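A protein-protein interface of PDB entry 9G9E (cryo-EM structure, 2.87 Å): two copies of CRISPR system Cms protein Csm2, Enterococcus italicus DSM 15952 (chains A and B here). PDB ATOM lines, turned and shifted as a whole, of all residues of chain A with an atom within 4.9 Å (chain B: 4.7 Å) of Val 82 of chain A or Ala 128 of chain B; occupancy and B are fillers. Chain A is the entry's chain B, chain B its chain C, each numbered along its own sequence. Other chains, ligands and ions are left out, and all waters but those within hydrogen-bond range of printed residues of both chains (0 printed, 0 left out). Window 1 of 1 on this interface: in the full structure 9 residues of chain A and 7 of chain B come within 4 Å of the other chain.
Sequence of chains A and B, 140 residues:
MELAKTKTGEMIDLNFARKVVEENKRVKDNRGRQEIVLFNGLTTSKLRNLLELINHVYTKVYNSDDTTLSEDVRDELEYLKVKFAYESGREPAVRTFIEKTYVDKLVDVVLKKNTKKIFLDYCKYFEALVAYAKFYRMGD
The side-chain amino group of Lys 83 of chain A sits at hydrogen-bond distance from the side-chain hydroxyl of Tyr 79 of chain A (3.3 Å).
Printed residues of chain B that touch a printed residue of chain A: Lys 124, Glu 127, Ala 128, Ala 131 and Tyr 132. Along chain B the printed residues that touch a printed residue of chain A span positions 124 to 132. Printed residues of chain A that touch a printed residue of chain B: Glu 78, Tyr 79, Val 82, Lys 83, Ala 85 and Tyr 86. Hydrophobic or aromatic side chains of chain A within 4 Å of the printed part of chain B: Tyr 79, Val 82, Ala 85 and Tyr 86. Along chain A the printed residues that touch a printed residue of chain B span positions 78 to 86. Among the printed residues, 7 pairs touch across the chains.
Tyr 79 of chain A touches Lys 124 of chain B. Val 82 of chain A touches Ala 128 of chain B. Tyr 132 of chain B touches Ala 85 of chain A. Tyr 86 of chain A touches Ala 131 of chain B (CB to CB, 3.99 Å).
No position is printed for both chains. Of the 7 pairs that touch across the chains among the printed residues, none has its exchanged pair printed and touching as well.
Of chain A, only Val 82 (3.5 Å) comes within 4 Å of Ala 128 of chain B. Of the printed residues of chain A, Glu 127 of chain B touches Tyr 79 and Lys 83. Of the printed residues of chain B, Glu 78 of chain A touches Lys 124 (3.6 Å). The nearest residue of chain B that does not touch Val 82 of chain A is Glu 127 of chain B (4.1 Å).
NZ of Lys 124 of chain B lies within salt-bridge range of OE2 of Glu 78 of chain A, at 3.6 Å. OE2 of Glu 127 of chain B sits at hydrogen-bond distance from OH of Tyr 79 of chain A (3.0 Å). The side-chain carboxylate (OE2) of Glu 127 of chain B lies within salt-bridge range of the side-chain amino group (NZ) of Lys 83 of chain A.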
ATOM      1  N   GLU A  78      27.645  16.844 -16.859  1.00  0.00           N
ATOM      2  CA  GLU A  78      26.662  15.871 -16.386  1.00  0.00           C
ATOM      3  C   GLU A  78      25.422  16.571 -15.835  1.00  0.00           C
ATOM      4  O   GLU A  78      24.287  16.143 -16.083  1.00  0.00           O
ATOM      5  CB  GLU A  78      27.288  14.969 -15.322  1.00  0.00           C
ATOM      6  CG  GLU A  78      27.655  13.580 -15.817  1.00  0.00           C
ATOM      7  CD  GLU A  78      28.157  12.680 -14.704  1.00  0.00           C
ATOM      8  OE1 GLU A  78      28.587  11.546 -15.002  1.00  0.00           O
ATOM      9  OE2 GLU A  78      28.120  13.106 -13.531  1.00  0.00           O
ATOM     10  N   TYR A  79      25.627  17.656 -15.085  1.00  0.00           N
ATOM     11  CA  TYR A  79      24.506  18.451 -14.594  1.00  0.00           C
ATOM     12  C   TYR A  79      23.723  19.068 -15.746  1.00  0.00           C
ATOM     13  O   TYR A  79      22.495  19.173 -15.687  1.00  0.00           O
ATOM     14  CB  TYR A  79      25.013  19.538 -13.645  1.00  0.00           C
ATOM     15  CG  TYR A  79      23.945  20.122 -12.752  1.00  0.00           C
ATOM     16  CD1 TYR A  79      23.630  19.531 -11.535  1.00  0.00           C
ATOM     17  CD2 TYR A  79      23.253  21.268 -13.122  1.00  0.00           C
ATOM     18  CE1 TYR A  79      22.654  20.063 -10.714  1.00  0.00           C
ATOM     19  CE2 TYR A  79      22.276  21.808 -12.309  1.00  0.00           C
ATOM     20  CZ  TYR A  79      21.980  21.201 -11.106  1.00  0.00           C
ATOM     21  OH  TYR A  79      21.008  21.734 -10.291  1.00  0.00           O
ATOM     22  N   LEU A  80      24.419  19.493 -16.800  1.00  0.00           N
ATOM     23  CA  LEU A  80      23.741  20.030 -17.974  1.00  0.00           C
ATOM     24  C   LEU A  80      22.910  18.955 -18.665  1.00  0.00           C
ATOM     25  O   LEU A  80      21.806  19.225 -19.145  1.00  0.00           O
ATOM     26  CB  LEU A  80      24.765  20.630 -18.937  1.00  0.00           C
ATOM     27  CG  LEU A  80      24.296  20.934 -20.358  1.00  0.00           C
ATOM     28  CD1 LEU A  80      23.276  22.064 -20.350  1.00  0.00           C
ATOM     29  CD2 LEU A  80      25.473  21.274 -21.258  1.00  0.00           C
ATOM     30  N   LYS A  81      23.431  17.728 -18.725  1.00  0.00           N
ATOM     31  CA  LYS A  81      22.663  16.618 -19.287  1.00  0.00           C
ATOM     32  C   LYS A  81      21.408  16.343 -18.468  1.00  0.00           C
ATOM     33  O   LYS A  81      20.322  16.123 -19.024  1.00  0.00           O
ATOM     34  CB  LYS A  81      23.535  15.365 -19.359  1.00  0.00           C
ATOM     35  CG  LYS A  81      22.840  14.157 -19.964  1.00  0.00           C
ATOM     36  CD  LYS A  81      23.786  12.972 -20.065  1.00  0.00           C
ATOM     37  CE  LYS A  81      24.268  12.535 -18.691  1.00  0.00           C
ATOM     38  NZ  LYS A  81      25.144  11.332 -18.761  1.00  0.00           N
ATOM     39  N   VAL A  82      21.534  16.347 -17.139  1.00  0.00           N
ATOM     40  CA  VAL A  82      20.352  16.095 -16.321  1.00  0.00           C
ATOM     41  C   VAL A  82      19.373  17.263 -16.414  1.00  0.00           C
ATOM     42  O   VAL A  82      18.157  17.067 -16.321  1.00  0.00           O
ATOM     43  CB  VAL A  82      20.734  15.774 -14.863  1.00  0.00           C
ATOM     44  CG1 VAL A  82      21.012  17.034 -14.063  1.00  0.00           C
ATOM     45  CG2 VAL A  82      19.628  14.974 -14.218  1.00  0.00           C
ATOM     46  N   LYS A  83      19.874  18.484 -16.618  1.00  0.00           N
ATOM     47  CA  LYS A  83      18.986  19.616 -16.865  1.00  0.00           C
ATOM     48  C   LYS A  83      18.267  19.464 -18.198  1.00  0.00           C
ATOM     49  O   LYS A  83      17.095  19.832 -18.323  1.00  0.00           O
ATOM     50  CB  LYS A  83      19.775  20.924 -16.822  1.00  0.00           C
ATOM     51  CG  LYS A  83      19.104  22.028 -16.023  1.00  0.00           C
ATOM     52  CD  LYS A  83      19.123  21.725 -14.534  1.00  0.00           C
ATOM     53  CE  LYS A  83      18.628  22.912 -13.724  1.00  0.00           C
ATOM     54  NZ  LYS A  83      18.479  22.579 -12.281  1.00  0.00           N
ATOM     55  N   PHE A  84      18.961  18.935 -19.208  1.00  0.00           N
ATOM     56  CA  PHE A  84      18.310  18.624 -20.476  1.00  0.00           C
ATOM     57  C   PHE A  84      17.174  17.634 -20.268  1.00  0.00           C
ATOM     58  O   PHE A  84      16.073  17.813 -20.802  1.00  0.00           O
ATOM     59  CB  PHE A  84      19.321  18.047 -21.468  1.00  0.00           C
ATOM     60  CG  PHE A  84      20.100  19.082 -22.226  1.00  0.00           C
ATOM     61  CD1 PHE A  84      19.453  20.074 -22.938  1.00  0.00           C
ATOM     62  CD2 PHE A  84      21.483  19.034 -22.262  1.00  0.00           C
ATOM     63  CE1 PHE A  84      20.167  21.018 -23.646  1.00  0.00           C
ATOM     64  CE2 PHE A  84      22.202  19.973 -22.972  1.00  0.00           C
ATOM     65  CZ  PHE A  84      21.545  20.968 -23.663  1.00  0.00           C
ATOM     66  N   ALA A  85      17.428  16.580 -19.489  1.00  0.00           N
ATOM     67  CA  ALA A  85      16.388  15.592 -19.212  1.00  0.00           C
ATOM     68  C   ALA A  85      15.218  16.214 -18.454  1.00  0.00           C
ATOM     69  O   ALA A  85      14.050  15.935 -18.757  1.00  0.00           O
ATOM     70  CB  ALA A  85      16.972  14.419 -18.428  1.00  0.00           C
ATOM     71  N   TYR A  86      15.515  17.059 -17.466  1.00  0.00           N
ATOM     72  CA  TYR A  86      14.465  17.709 -16.687  1.00  0.00           C
ATOM     73  C   TYR A  86      13.612  18.624 -17.558  1.00  0.00           C
ATOM     74  O   TYR A  86      12.382  18.645 -17.432  1.00  0.00           O
ATOM     75  CB  TYR A  86      15.093  18.488 -15.530  1.00  0.00           C
ATOM     76  CG  TYR A  86      14.154  19.425 -14.808  1.00  0.00           C
ATOM     77  CD1 TYR A  86      13.199  18.939 -13.924  1.00  0.00           C
ATOM     78  CD2 TYR A  86      14.235  20.799 -14.994  1.00  0.00           C
ATOM     79  CE1 TYR A  86      12.343  19.794 -13.256  1.00  0.00           C
ATOM     80  CE2 TYR A  86      13.383  21.661 -14.332  1.00  0.00           C
ATOM     81  CZ  TYR A  86      12.440  21.154 -13.463  1.00  0.00           C
ATOM     82  OH  TYR A  86      11.591  22.011 -12.801  1.00  0.00           O
ATOM     83  N   ALA B  17      21.989   7.197 -12.398  1.00  0.00           N
ATOM     84  CA  ALA B  17      20.585   7.109 -12.020  1.00  0.00           C
ATOM     85  C   ALA B  17      19.684   6.737 -13.190  1.00  0.00           C
ATOM     86  O   ALA B  17      18.524   6.375 -12.964  1.00  0.00           O
ATOM     87  CB  ALA B  17      20.121   8.434 -11.413  1.00  0.00           C
ATOM     88  N   LYS B 124      22.671  16.365  -5.934  1.00  0.00           N
ATOM     89  CA  LYS B 124      22.579  16.367  -7.389  1.00  0.00           C
ATOM     90  C   LYS B 124      22.140  15.002  -7.905  1.00  0.00           C
ATOM     91  O   LYS B 124      21.354  14.915  -8.851  1.00  0.00           O
ATOM     92  CB  LYS B 124      23.924  16.816  -7.985  1.00  0.00           C
ATOM     93  CG  LYS B 124      24.202  16.566  -9.484  1.00  0.00           C
ATOM     94  CD  LYS B 124      24.524  15.120  -9.861  1.00  0.00           C
ATOM     95  CE  LYS B 124      24.805  14.990 -11.349  1.00  0.00           C
ATOM     96  NZ  LYS B 124      25.058  13.579 -11.743  1.00  0.00           N
ATOM     97  N   TYR B 125      22.637  13.923  -7.294  1.00  0.00           N
ATOM     98  CA  TYR B 125      22.221  12.582  -7.698  1.00  0.00           C
ATOM     99  C   TYR B 125      20.740  12.349  -7.420  1.00  0.00           C
ATOM    100  O   TYR B 125      20.032  11.758  -8.243  1.00  0.00           O
ATOM    101  CB  TYR B 125      23.075  11.536  -6.984  1.00  0.00           C
ATOM    102  CG  TYR B 125      22.519  10.131  -7.057  1.00  0.00           C
ATOM    103  CD1 TYR B 125      22.435   9.458  -8.268  1.00  0.00           C
ATOM    104  CD2 TYR B 125      22.082   9.477  -5.912  1.00  0.00           C
ATOM    105  CE1 TYR B 125      21.929   8.174  -8.338  1.00  0.00           C
ATOM    106  CE2 TYR B 125      21.575   8.194  -5.972  1.00  0.00           C
ATOM    107  CZ  TYR B 125      21.502   7.546  -7.188  1.00  0.00           C
ATOM    108  OH  TYR B 125      20.997   6.268  -7.252  1.00  0.00           O
ATOM    109  N   PHE B 126      20.255  12.800  -6.262  1.00  0.00           N
ATOM    110  CA  PHE B 126      18.841  12.633  -5.938  1.00  0.00           C
ATOM    111  C   PHE B 126      17.967  13.473  -6.865  1.00  0.00           C
ATOM    112  O   PHE B 126      16.898  13.030  -7.311  1.00  0.00           O
ATOM    113  CB  PHE B 126      18.603  12.999  -4.473  1.00  0.00           C
ATOM    114  CG  PHE B 126      17.216  12.703  -3.991  1.00  0.00           C
ATOM    115  CD1 PHE B 126      16.837  11.405  -3.691  1.00  0.00           C
ATOM    116  CD2 PHE B 126      16.293  13.720  -3.826  1.00  0.00           C
ATOM    117  CE1 PHE B 126      15.561  11.127  -3.243  1.00  0.00           C
ATOM    118  CE2 PHE B 126      15.020  13.448  -3.378  1.00  0.00           C
ATOM    119  CZ  PHE B 126      14.651  12.151  -3.086  1.00  0.00           C
ATOM    120  N   GLU B 127      18.411  14.696  -7.168  1.00  0.00           N
ATOM    121  CA  GLU B 127      17.715  15.525  -8.144  1.00  0.00           C
ATOM    122  C   GLU B 127      17.700  14.859  -9.512  1.00  0.00           C
ATOM    123  O   GLU B 127      16.702  14.929 -10.233  1.00  0.00           O
ATOM    124  CB  GLU B 127      18.371  16.905  -8.219  1.00  0.00           C
ATOM    125  CG  GLU B 127      18.299  17.564  -9.586  1.00  0.00           C
ATOM    126  CD  GLU B 127      19.173  18.797  -9.685  1.00  0.00           C
ATOM    127  OE1 GLU B 127      19.425  19.435  -8.641  1.00  0.00           O
ATOM    128  OE2 GLU B 127      19.610  19.129 -10.807  1.00  0.00           O
ATOM    129  N   ALA B 128      18.802  14.204  -9.884  1.00  0.00           N
ATOM    130  CA  ALA B 128      18.841  13.455 -11.134  1.00  0.00           C
ATOM    131  C   ALA B 128      17.834  12.317 -11.122  1.00  0.00           C
ATOM    132  O   ALA B 128      17.167  12.055 -12.129  1.00  0.00           O
ATOM    133  CB  ALA B 128      20.252  12.918 -11.377  1.00  0.00           C
ATOM    134  N   LEU B 129      17.720  11.623  -9.989  1.00  0.00           N
ATOM    135  CA  LEU B 129      16.737  10.550  -9.868  1.00  0.00           C
ATOM    136  C   LEU B 129      15.324  11.075 -10.092  1.00  0.00           C
ATOM    137  O   LEU B 129      14.562  10.527 -10.900  1.00  0.00           O
ATOM    138  CB  LEU B 129      16.852   9.892  -8.492  1.00  0.00           C
ATOM    139  CG  LEU B 129      17.891   8.784  -8.331  1.00  0.00           C
ATOM    140  CD1 LEU B 129      18.122   8.490  -6.858  1.00  0.00           C
ATOM    141  CD2 LEU B 129      17.453   7.529  -9.066  1.00  0.00           C
ATOM    142  N   VAL B 130      14.959  12.154  -9.392  1.00  0.00           N
ATOM    143  CA  VAL B 130      13.603  12.685  -9.524  1.00  0.00           C
ATOM    144  C   VAL B 130      13.377  13.262 -10.921  1.00  0.00           C
ATOM    145  O   VAL B 130      12.273  13.167 -11.472  1.00  0.00           O
ATOM    146  CB  VAL B 130      13.297  13.708  -8.411  1.00  0.00           C
ATOM    147  CG1 VAL B 130      13.805  13.204  -7.071  1.00  0.00           C
ATOM    148  CG2 VAL B 130      13.892  15.074  -8.724  1.00  0.00           C
ATOM    149  N   ALA B 131      14.415  13.843 -11.528  1.00  0.00           N
ATOM    150  CA  ALA B 131      14.273  14.406 -12.867  1.00  0.00           C
ATOM    151  C   ALA B 131      14.074  13.314 -13.908  1.00  0.00           C
ATOM    152  O   ALA B 131      13.247  13.457 -14.813  1.00  0.00           O
ATOM    153  CB  ALA B 131      15.492  15.261 -13.210  1.00  0.00           C
ATOM    154  N   TYR B 132      14.826  12.216 -13.800  1.00  0.00           N
ATOM    155  CA  TYR B 132      14.626  11.093 -14.708  1.00  0.00           C
ATOM    156  C   TYR B 132      13.259  10.458 -14.496  1.00  0.00           C
ATOM    157  O   TYR B 132      12.617  10.019 -15.457  1.00  0.00           O
ATOM    158  CB  TYR B 132      15.737  10.061 -14.522  1.00  0.00           C
ATOM    159  CG  TYR B 132      17.068  10.479 -15.105  1.00  0.00           C
ATOM    160  CD1 TYR B 132      17.135  11.168 -16.309  1.00  0.00           C
ATOM    161  CD2 TYR B 132      18.257  10.186 -14.451  1.00  0.00           C
ATOM    162  CE1 TYR B 132      18.349  11.553 -16.845  1.00  0.00           C
ATOM    163  CE2 TYR B 132      19.475  10.568 -14.979  1.00  0.00           C
ATOM    164  CZ  TYR B 132      19.516  11.250 -16.175  1.00  0.00           C
ATOM    165  OH  TYR B 132      20.727  11.631 -16.705  1.00  0.00           O
